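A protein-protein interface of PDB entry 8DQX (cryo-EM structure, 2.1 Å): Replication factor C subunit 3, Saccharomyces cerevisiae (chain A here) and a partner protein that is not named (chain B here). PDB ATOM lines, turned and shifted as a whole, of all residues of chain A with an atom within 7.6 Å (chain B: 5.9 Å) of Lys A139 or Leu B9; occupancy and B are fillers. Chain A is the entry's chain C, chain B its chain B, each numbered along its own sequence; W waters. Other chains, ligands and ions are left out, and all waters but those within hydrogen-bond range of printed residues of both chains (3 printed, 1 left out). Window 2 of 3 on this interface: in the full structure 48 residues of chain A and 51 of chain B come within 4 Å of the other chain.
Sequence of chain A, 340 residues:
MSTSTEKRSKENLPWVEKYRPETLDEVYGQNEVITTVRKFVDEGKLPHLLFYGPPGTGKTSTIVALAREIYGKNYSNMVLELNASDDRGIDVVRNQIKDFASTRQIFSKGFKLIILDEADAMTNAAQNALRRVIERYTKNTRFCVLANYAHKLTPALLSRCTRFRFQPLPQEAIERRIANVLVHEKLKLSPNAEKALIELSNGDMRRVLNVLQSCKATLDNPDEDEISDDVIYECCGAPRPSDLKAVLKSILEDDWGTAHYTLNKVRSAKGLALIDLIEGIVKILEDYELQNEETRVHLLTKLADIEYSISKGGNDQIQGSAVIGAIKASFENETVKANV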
ATOM      1  N   GLY A  44       9.279 -21.475  -3.064  1.00  0.00           N
ATOM      2  CA  GLY A  44      10.414 -21.604  -3.954  1.00  0.00           C
ATOM      3  C   GLY A  44      11.032 -20.296  -4.387  1.00  0.00           C
ATOM      4  O   GLY A  44      11.831 -20.290  -5.330  1.00  0.00           O
ATOM      5  N   LYS A  45      10.685 -19.188  -3.736  1.00  0.00           N
ATOM      6  CA  LYS A  45      11.213 -17.865  -4.059  1.00  0.00           C
ATOM      7  C   LYS A  45      12.171 -17.448  -2.946  1.00  0.00           C
ATOM      8  O   LYS A  45      11.769 -16.806  -1.975  1.00  0.00           O
ATOM      9  CB  LYS A  45      10.089 -16.846  -4.218  1.00  0.00           C
ATOM     10  CG  LYS A  45       9.074 -17.175  -5.299  1.00  0.00           C
ATOM     11  CD  LYS A  45       7.900 -16.214  -5.238  1.00  0.00           C
ATOM     12  CE  LYS A  45       8.245 -14.870  -5.853  1.00  0.00           C
ATOM     13  NZ  LYS A  45       7.044 -14.004  -6.000  1.00  0.00           N
ATOM     14  N   LEU A  46      13.440 -17.812  -3.094  1.00  0.00           N
ATOM     15  CA  LEU A  46      14.477 -17.388  -2.162  1.00  0.00           C
ATOM     16  C   LEU A  46      15.320 -16.296  -2.802  1.00  0.00           C
ATOM     17  O   LEU A  46      16.073 -16.582  -3.744  1.00  0.00           O
ATOM     18  CB  LEU A  46      15.364 -18.567  -1.756  1.00  0.00           C
ATOM     19  CG  LEU A  46      16.231 -18.349  -0.511  1.00  0.00           C
ATOM     20  CD1 LEU A  46      15.394 -17.981   0.702  1.00  0.00           C
ATOM     21  CD2 LEU A  46      17.084 -19.573  -0.224  1.00  0.00           C
ATOM     22  N   PRO A  47      15.243 -15.052  -2.351  1.00  0.00           N
ATOM     23  CA  PRO A  47      16.136 -14.015  -2.870  1.00  0.00           C
ATOM     24  C   PRO A  47      17.467 -14.032  -2.123  1.00  0.00           C
ATOM     25  O   PRO A  47      17.676 -14.803  -1.190  1.00  0.00           O
ATOM     26  CB  PRO A  47      15.353 -12.728  -2.615  1.00  0.00           C
ATOM     27  CG  PRO A  47      14.555 -13.019  -1.385  1.00  0.00           C
ATOM     28  CD  PRO A  47      14.297 -14.513  -1.359  1.00  0.00           C
ATOM     29  N   HIS A  48      18.381 -13.176  -2.567  1.00  0.00           N
ATOM     30  CA  HIS A  48      19.614 -12.949  -1.826  1.00  0.00           C
ATOM     31  C   HIS A  48      19.287 -12.219  -0.525  1.00  0.00           C
ATOM     32  O   HIS A  48      18.640 -11.169  -0.543  1.00  0.00           O
ATOM     33  CB  HIS A  48      20.594 -12.134  -2.672  1.00  0.00           C
ATOM     34  CG  HIS A  48      20.884 -12.733  -4.015  1.00  0.00           C
ATOM     35  ND1 HIS A  48      21.585 -13.908  -4.172  1.00  0.00           N
ATOM     36  CD2 HIS A  48      20.568 -12.316  -5.265  1.00  0.00           C
ATOM     37  CE1 HIS A  48      21.692 -14.190  -5.457  1.00  0.00           C
ATOM     38  NE2 HIS A  48      21.079 -13.241  -6.142  1.00  0.00           N
ATOM     39  N   ALA A 101      29.594 -21.322  -7.058  1.00  0.00           N
ATOM     40  CA  ALA A 101      28.384 -20.699  -7.588  1.00  0.00           C
ATOM     41  C   ALA A 101      28.039 -21.210  -8.982  1.00  0.00           C
ATOM     42  O   ALA A 101      26.858 -21.302  -9.326  1.00  0.00           O
ATOM     43  CB  ALA A 101      28.544 -19.180  -7.609  1.00  0.00           C
ATOM     44  N   PHE A 111      19.614 -26.261  -6.190  1.00  0.00           N
ATOM     45  CA  PHE A 111      20.295 -24.976  -6.209  1.00  0.00           C
ATOM     46  C   PHE A 111      21.333 -24.896  -5.094  1.00  0.00           C
ATOM     47  O   PHE A 111      21.284 -25.633  -4.106  1.00  0.00           O
ATOM     48  CB  PHE A 111      19.285 -23.841  -6.070  1.00  0.00           C
ATOM     49  CG  PHE A 111      18.884 -23.555  -4.650  1.00  0.00           C
ATOM     50  CD1 PHE A 111      17.929 -24.337  -4.013  1.00  0.00           C
ATOM     51  CD2 PHE A 111      19.449 -22.499  -3.956  1.00  0.00           C
ATOM     52  CE1 PHE A 111      17.553 -24.068  -2.715  1.00  0.00           C
ATOM     53  CE2 PHE A 111      19.077 -22.226  -2.659  1.00  0.00           C
ATOM     54  CZ  PHE A 111      18.129 -23.011  -2.035  1.00  0.00           C
ATOM     55  N   LYS A 112      22.280 -23.976  -5.263  1.00  0.00           N
ATOM     56  CA  LYS A 112      23.377 -23.785  -4.327  1.00  0.00           C
ATOM     57  C   LYS A 112      23.060 -22.645  -3.361  1.00  0.00           C
ATOM     58  O   LYS A 112      22.393 -21.672  -3.717  1.00  0.00           O
ATOM     59  CB  LYS A 112      24.686 -23.477  -5.064  1.00  0.00           C
ATOM     60  CG  LYS A 112      24.907 -24.230  -6.383  1.00  0.00           C
ATOM     61  CD  LYS A 112      25.198 -25.706  -6.169  1.00  0.00           C
ATOM     62  CE  LYS A 112      26.607 -25.941  -5.642  1.00  0.00           C
ATOM     63  NZ  LYS A 112      27.642 -25.962  -6.702  1.00  0.00           N
ATOM     64  N   ILE A 134      27.295 -12.499  -7.742  1.00  0.00           N
ATOM     65  CA  ILE A 134      25.937 -12.604  -7.216  1.00  0.00           C
ATOM     66  C   ILE A 134      24.924 -12.466  -8.344  1.00  0.00           C
ATOM     67  O   ILE A 134      23.975 -13.251  -8.448  1.00  0.00           O
ATOM     68  CB  ILE A 134      25.697 -11.552  -6.118  1.00  0.00           C
ATOM     69  CG1 ILE A 134      26.529 -11.869  -4.873  1.00  0.00           C
ATOM     70  CG2 ILE A 134      24.206 -11.477  -5.767  1.00  0.00           C
ATOM     71  CD1 ILE A 134      26.560 -10.738  -3.866  1.00  0.00           C
ATOM     72  N   GLU A 135      25.111 -11.467  -9.211  1.00  0.00           N
ATOM     73  CA  GLU A 135      24.114 -11.233 -10.258  1.00  0.00           C
ATOM     74  C   GLU A 135      24.141 -12.317 -11.339  1.00  0.00           C
ATOM     75  O   GLU A 135      23.084 -12.761 -11.796  1.00  0.00           O
ATOM     76  CB  GLU A 135      24.313  -9.851 -10.880  1.00  0.00           C
ATOM     77  CG  GLU A 135      23.690  -8.732 -10.068  1.00  0.00           C
ATOM     78  CD  GLU A 135      23.858  -7.368 -10.713  1.00  0.00           C
ATOM     79  OE1 GLU A 135      24.928  -7.110 -11.301  1.00  0.00           O
ATOM     80  OE2 GLU A 135      22.916  -6.557 -10.628  1.00  0.00           O
ATOM     81  N   ARG A 136      25.329 -12.758 -11.756  1.00  0.00           N
ATOM     82  CA  ARG A 136      25.429 -13.631 -12.925  1.00  0.00           C
ATOM     83  C   ARG A 136      24.892 -15.035 -12.661  1.00  0.00           C
ATOM     84  O   ARG A 136      24.322 -15.654 -13.565  1.00  0.00           O
ATOM     85  CB  ARG A 136      26.886 -13.697 -13.393  1.00  0.00           C
ATOM     86  CG  ARG A 136      27.197 -14.831 -14.364  1.00  0.00           C
ATOM     87  CD  ARG A 136      28.641 -14.783 -14.827  1.00  0.00           C
ATOM     88  NE  ARG A 136      28.947 -15.840 -15.784  1.00  0.00           N
ATOM     89  CZ  ARG A 136      29.016 -15.682 -17.100  1.00  0.00           C
ATOM     90  NH1 ARG A 136      28.792 -14.509 -17.671  1.00  0.00           N
ATOM     91  NH2 ARG A 136      29.316 -16.728 -17.863  1.00  0.00           N
ATOM     92  N   TYR A 137      25.067 -15.564 -11.449  1.00  0.00           N
ATOM     93  CA  TYR A 137      24.698 -16.943 -11.151  1.00  0.00           C
ATOM     94  C   TYR A 137      23.436 -17.038 -10.301  1.00  0.00           C
ATOM     95  O   TYR A 137      23.235 -18.035  -9.602  1.00  0.00           O
ATOM     96  CB  TYR A 137      25.865 -17.654 -10.469  1.00  0.00           C
ATOM     97  CG  TYR A 137      27.080 -17.705 -11.352  1.00  0.00           C
ATOM     98  CD1 TYR A 137      27.077 -18.454 -12.519  1.00  0.00           C
ATOM     99  CD2 TYR A 137      28.217 -16.971 -11.046  1.00  0.00           C
ATOM    100  CE1 TYR A 137      28.178 -18.491 -13.345  1.00  0.00           C
ATOM    101  CE2 TYR A 137      29.324 -17.003 -11.864  1.00  0.00           C
ATOM    102  CZ  TYR A 137      29.297 -17.764 -13.013  1.00  0.00           C
ATOM    103  OH  TYR A 137      30.395 -17.799 -13.833  1.00  0.00           O
ATOM    104  N   THR A 138      22.573 -16.023 -10.366  1.00  0.00           N
ATOM    105  CA  THR A 138      21.359 -16.023  -9.559  1.00  0.00           C
ATOM    106  C   THR A 138      20.459 -17.206  -9.890  1.00  0.00           C
ATOM    107  O   THR A 138      19.778 -17.728  -9.005  1.00  0.00           O
ATOM    108  CB  THR A 138      20.602 -14.707  -9.761  1.00  0.00           C
ATOM    109  OG1 THR A 138      21.365 -13.626  -9.215  1.00  0.00           O
ATOM    110  CG2 THR A 138      19.237 -14.746  -9.089  1.00  0.00           C
ATOM    111  N   LYS A 139      20.438 -17.642 -11.152  1.00  0.00           N
ATOM    112  CA  LYS A 139      19.493 -18.681 -11.548  1.00  0.00           C
ATOM    113  C   LYS A 139      19.666 -19.938 -10.702  1.00  0.00           C
ATOM    114  O   LYS A 139      18.683 -20.597 -10.351  1.00  0.00           O
ATOM    115  CB  LYS A 139      19.659 -19.007 -13.031  1.00  0.00           C
ATOM    116  CG  LYS A 139      18.612 -19.965 -13.576  1.00  0.00           C
ATOM    117  CD  LYS A 139      19.065 -20.603 -14.882  1.00  0.00           C
ATOM    118  CE  LYS A 139      17.903 -21.218 -15.649  1.00  0.00           C
ATOM    119  NZ  LYS A 139      16.733 -21.526 -14.777  1.00  0.00           N
ATOM    120  N   ASN A 140      20.904 -20.277 -10.352  1.00  0.00           N
ATOM    121  CA  ASN A 140      21.178 -21.516  -9.643  1.00  0.00           C
ATOM    122  C   ASN A 140      21.729 -21.320  -8.236  1.00  0.00           C
ATOM    123  O   ASN A 140      21.795 -22.295  -7.483  1.00  0.00           O
ATOM    124  CB  ASN A 140      22.159 -22.365 -10.460  1.00  0.00           C
ATOM    125  CG  ASN A 140      21.538 -22.892 -11.743  1.00  0.00           C
ATOM    126  OD1 ASN A 140      22.074 -22.695 -12.834  1.00  0.00           O
ATOM    127  ND2 ASN A 140      20.396 -23.548 -11.619  1.00  0.00           N
ATOM    128  N   THR A 141      22.109 -20.099  -7.855  1.00  0.00           N
ATOM    129  CA  THR A 141      22.781 -19.850  -6.585  1.00  0.00           C
ATOM    130  C   THR A 141      22.152 -18.663  -5.867  1.00  0.00           C
ATOM    131  O   THR A 141      21.782 -17.670  -6.500  1.00  0.00           O
ATOM    132  CB  THR A 141      24.276 -19.571  -6.797  1.00  0.00           C
ATOM    133  OG1 THR A 141      24.880 -20.673  -7.483  1.00  0.00           O
ATOM    134  CG2 THR A 141      24.981 -19.345  -5.463  1.00  0.00           C
ATOM    135  N   ARG A 142      22.057 -18.763  -4.542  1.00  0.00           N
ATOM    136  CA  ARG A 142      21.588 -17.670  -3.700  1.00  0.00           C
ATOM    137  C   ARG A 142      22.562 -17.420  -2.561  1.00  0.00           C
ATOM    138  O   ARG A 142      23.071 -18.360  -1.946  1.00  0.00           O
ATOM    139  CB  ARG A 142      20.189 -17.950  -3.131  1.00  0.00           C
ATOM    140  CG  ARG A 142      19.162 -18.308  -4.186  1.00  0.00           C
ATOM    141  CD  ARG A 142      18.900 -17.146  -5.129  1.00  0.00           C
ATOM    142  NE  ARG A 142      18.602 -17.610  -6.475  1.00  0.00           N
ATOM    143  CZ  ARG A 142      17.392 -17.930  -6.907  1.00  0.00           C
ATOM    144  NH1 ARG A 142      16.325 -17.805  -6.134  1.00  0.00           N
ATOM    145  NH2 ARG A 142      17.246 -18.384  -8.148  1.00  0.00           N
ATOM    146  N   LEU B   7      14.949 -23.470  -7.920  1.00  0.00           N
ATOM    147  CA  LEU B   7      14.306 -22.236  -7.487  1.00  0.00           C
ATOM    148  C   LEU B   7      13.800 -21.409  -8.660  1.00  0.00           C
ATOM    149  O   LEU B   7      14.245 -21.572  -9.794  1.00  0.00           O
ATOM    150  CB  LEU B   7      15.278 -21.390  -6.657  1.00  0.00           C
ATOM    151  CG  LEU B   7      15.145 -21.515  -5.139  1.00  0.00           C
ATOM    152  CD1 LEU B   7      15.004 -22.967  -4.724  1.00  0.00           C
ATOM    153  CD2 LEU B   7      16.327 -20.869  -4.448  1.00  0.00           C
ATOM    154  N   GLN B   8      12.866 -20.515  -8.367  1.00  0.00           N
ATOM    155  CA  GLN B   8      12.386 -19.542  -9.334  1.00  0.00           C
ATOM    156  C   GLN B   8      13.201 -18.258  -9.238  1.00  0.00           C
ATOM    157  O   GLN B   8      13.740 -17.910  -8.186  1.00  0.00           O
ATOM    158  CB  GLN B   8      10.906 -19.243  -9.103  1.00  0.00           C
ATOM    159  CG  GLN B   8       9.973 -20.302  -9.658  1.00  0.00           C
ATOM    160  CD  GLN B   8       8.538 -19.826  -9.737  1.00  0.00           C
ATOM    161  OE1 GLN B   8       7.848 -20.061 -10.729  1.00  0.00           O
ATOM    162  NE2 GLN B   8       8.078 -19.153  -8.688  1.00  0.00           N
ATOM    163  N   LEU B   9      13.283 -17.554 -10.358  1.00  0.00           N
ATOM    164  CA  LEU B   9      14.098 -16.354 -10.421  1.00  0.00           C
ATOM    165  C   LEU B   9      13.558 -15.292  -9.462  1.00  0.00           C
ATOM    166  O   LEU B   9      12.347 -15.074  -9.395  1.00  0.00           O
ATOM    167  CB  LEU B   9      14.112 -15.794 -11.844  1.00  0.00           C
ATOM    168  CG  LEU B   9      15.230 -16.206 -12.810  1.00  0.00           C
ATOM    169  CD1 LEU B   9      15.299 -15.206 -13.946  1.00  0.00           C
ATOM    170  CD2 LEU B   9      16.587 -16.323 -12.127  1.00  0.00           C
ATOM    171  N   PRO B  10      14.427 -14.610  -8.717  1.00  0.00           N
ATOM    172  CA  PRO B  10      13.979 -13.410  -8.002  1.00  0.00           C
ATOM    173  C   PRO B  10      13.470 -12.374  -8.990  1.00  0.00           C
ATOM    174  O   PRO B  10      13.930 -12.297 -10.129  1.00  0.00           O
ATOM    175  CB  PRO B  10      15.235 -12.919  -7.273  1.00  0.00           C
ATOM    176  CG  PRO B  10      16.237 -13.984  -7.377  1.00  0.00           C
ATOM    177  CD  PRO B  10      15.822 -14.969  -8.413  1.00  0.00           C
ATOM    178  N   TRP B  11      12.499 -11.577  -8.543  1.00  0.00           N
ATOM    179  CA  TRP B  11      11.876 -10.610  -9.441  1.00  0.00           C
ATOM    180  C   TRP B  11      12.898  -9.636 -10.013  1.00  0.00           C
ATOM    181  O   TRP B  11      12.759  -9.197 -11.161  1.00  0.00           O
ATOM    182  CB  TRP B  11      10.769  -9.853  -8.705  1.00  0.00           C
ATOM    183  CG  TRP B  11       9.492 -10.632  -8.551  1.00  0.00           C
ATOM    184  CD1 TRP B  11       9.207 -11.867  -9.069  1.00  0.00           C
ATOM    185  CD2 TRP B  11       8.325 -10.229  -7.821  1.00  0.00           C
ATOM    186  NE1 TRP B  11       7.940 -12.252  -8.708  1.00  0.00           N
ATOM    187  CE2 TRP B  11       7.377 -11.267  -7.941  1.00  0.00           C
ATOM    188  CE3 TRP B  11       7.991  -9.094  -7.080  1.00  0.00           C
ATOM    189  CZ2 TRP B  11       6.120 -11.199  -7.350  1.00  0.00           C
ATOM    190  CZ3 TRP B  11       6.744  -9.031  -6.492  1.00  0.00           C
ATOM    191  CH2 TRP B  11       5.823 -10.076  -6.630  1.00  0.00           C
ATOM    192  N   GLU B  13      15.886 -10.221 -11.040  1.00  0.00           N
ATOM    193  CA  GLU B  13      16.447 -10.817 -12.243  1.00  0.00           C
ATOM    194  C   GLU B  13      15.365 -11.208 -13.240  1.00  0.00           C
ATOM    195  O   GLU B  13      15.582 -11.106 -14.451  1.00  0.00           O
ATOM    196  CB  GLU B  13      17.298 -12.034 -11.881  1.00  0.00           C
ATOM    197  CG  GLU B  13      18.627 -11.672 -11.231  1.00  0.00           C
ATOM    198  CD  GLU B  13      19.506 -10.814 -12.131  1.00  0.00           C
ATOM    199  OE1 GLU B  13      19.342 -10.886 -13.368  1.00  0.00           O
ATOM    200  OE2 GLU B  13      20.356 -10.072 -11.602  1.00  0.00           O
ATOM    201  N   LYS B  14      14.197 -11.635 -12.758  1.00  0.00           N
ATOM    202  CA  LYS B  14      13.130 -12.025 -13.674  1.00  0.00           C
ATOM    203  C   LYS B  14      12.695 -10.854 -14.545  1.00  0.00           C
ATOM    204  O   LYS B  14      12.414 -11.030 -15.735  1.00  0.00           O
ATOM    205  CB  LYS B  14      11.941 -12.583 -12.895  1.00  0.00           C
ATOM    206  CG  LYS B  14      10.796 -13.032 -13.784  1.00  0.00           C
ATOM    207  CD  LYS B  14       9.753 -13.819 -13.005  1.00  0.00           C
ATOM    208  CE  LYS B  14       8.533 -14.106 -13.854  1.00  0.00           C
ATOM    209  NZ  LYS B  14       7.344 -14.472 -13.039  1.00  0.00           N
ATOM    210  N   GLN B 210       8.801  -7.729  -3.479  1.00  0.00           N
ATOM    211  CA  GLN B 210       8.763  -9.179  -3.316  1.00  0.00           C
ATOM    212  C   GLN B 210       8.667  -9.569  -1.849  1.00  0.00           C
ATOM    213  O   GLN B 210       7.888 -10.456  -1.487  1.00  0.00           O
ATOM    214  CB  GLN B 210       9.993  -9.827  -3.952  1.00  0.00           C
ATOM    215  CG  GLN B 210       9.710 -11.208  -4.521  1.00  0.00           C
ATOM    216  CD  GLN B 210      10.850 -11.772  -5.346  1.00  0.00           C
ATOM    217  OE1 GLN B 210      10.638 -12.418  -6.372  1.00  0.00           O
ATOM    218  NE2 GLN B 210      12.072 -11.479  -4.924  1.00  0.00           N
HETATM  219  O   HOH W   1      17.816 -23.189  -9.570  1.00  0.00           O
HETATM  220  O   HOH W   2      16.445 -26.334  -6.719  1.00  0.00           O
HETATM  221  O   HOH W   3      16.095 -19.613 -10.444  1.00  0.00           O
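Water W3 lies within hydrogen-bond range of O of Lys A139 (2.8 Å), O of Leu B7 (2.8 Å), NH2 of Arg A142 (2.8 Å) and N of Leu B9 (3.5 Å). Water W1 lies within hydrogen-bond range of the backbone carbonyl oxygen (O) of Lys A139 (2.8 Å), the side-chain amide nitrogen (ND2) of Asn A140 (3.3 Å) and the backbone NH (N) of Leu B7 (3.3 Å). Water W2 bridges the backbone NH (N) of Phe A111 (3.2 Å) and the backbone NH (N) of Leu B7 (3.4 Å).
Of the 17 printed residues of chain A, 8 touch a printed residue of chain B. Printed residues of chain A that touch a printed residue of chain B: Gly A44, Lys A45, Leu A46, Phe A111, Glu A135, Thr A138, Lys A139 and Arg A142. Of the 8 printed residues of chain B, 7 touch a printed residue of chain A. Hydrophobic or aromatic side chains of chain B that line the printed part of chain A: Leu B7, Leu B9, Pro B10 and Trp B11. Among the printed residues, no Asp or Glu carboxylate lies within 4 Å of a Lys or Arg side-chain nitrogen of the other chain.
The backbone NH of Gln B8 is in hydrogen-bond range of the backbone carbonyl oxygen of Gly A44 (3.2 Å). The guanidinium group of Arg A142 lies within hydrogen-bond range of the backbone carbonyl oxygen of Gln B8 (3.3 Å). NE1 of Trp B11 lies close to NZ of Lys A45 (3.3 Å).
NH1 of Arg A142 sits at hydrogen-bond distance from O of Leu A46 (2.7 Å). The side-chain hydroxyl of Thr A138 is in hydrogen-bond range of a ring nitrogen (NE2) of His A48 (3.1 Å). The backbone NH of Arg A142 lies within hydrogen-bond range of the backbone carbonyl oxygen of Lys A112 (3.0 Å). The backbone carbonyl oxygen (O) of Ile A134 sits at hydrogen-bond distance from the side-chain hydroxyl (OG1) of Thr A138 (2.7 Å). O of Glu A135 is in hydrogen-bond range of OG1 of Thr A138, 3.2 Å away. The backbone carbonyl oxygen of Lys A139 lies within hydrogen-bond range of the guanidinium group of Arg A142 (3.4 Å).
CG of Leu B7 touches O of Gly A44, at 3.5 Å. Gln B210 touches Lys A45. CB of Leu A46 touches CD2 of Leu B7, at 3.7 Å. Phe A111 touches Leu B7. Glu B13 touches Glu A135. CG2 of Thr A138 touches CD of Pro B10, 3.5 Å away. CG of Glu B13 touches CG2 of Thr A138 (3.8 Å). Lys A139 touches Leu B9. Leu B7 touches Arg A142 (CD2 to NH1, 3.5 Å). NH1 of Arg A142 touches CD of Pro B10 (3.7 Å).
Lys A139 touches just one residue of chain B: Leu B9. Leu B9 touches just one residue of chain A: Lys A139 (3.8 Å). Of the printed residues of chain B, Phe A111 touches Leu B7 (3.3 Å). Of the printed residues of chain A, Gln B210 touches Lys A45. Ile A134 touches none of the printed residues of chain B. The nearest residue of chain B that does not touch Lys A139 is Leu B7 (4.6 Å). The nearest residue of chain A that does not touch Leu B9 is Thr A138 (4.3 Å). The nearest printed residue of chain A that does not touch Gln B8 is Lys A45 (4.05 Å).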
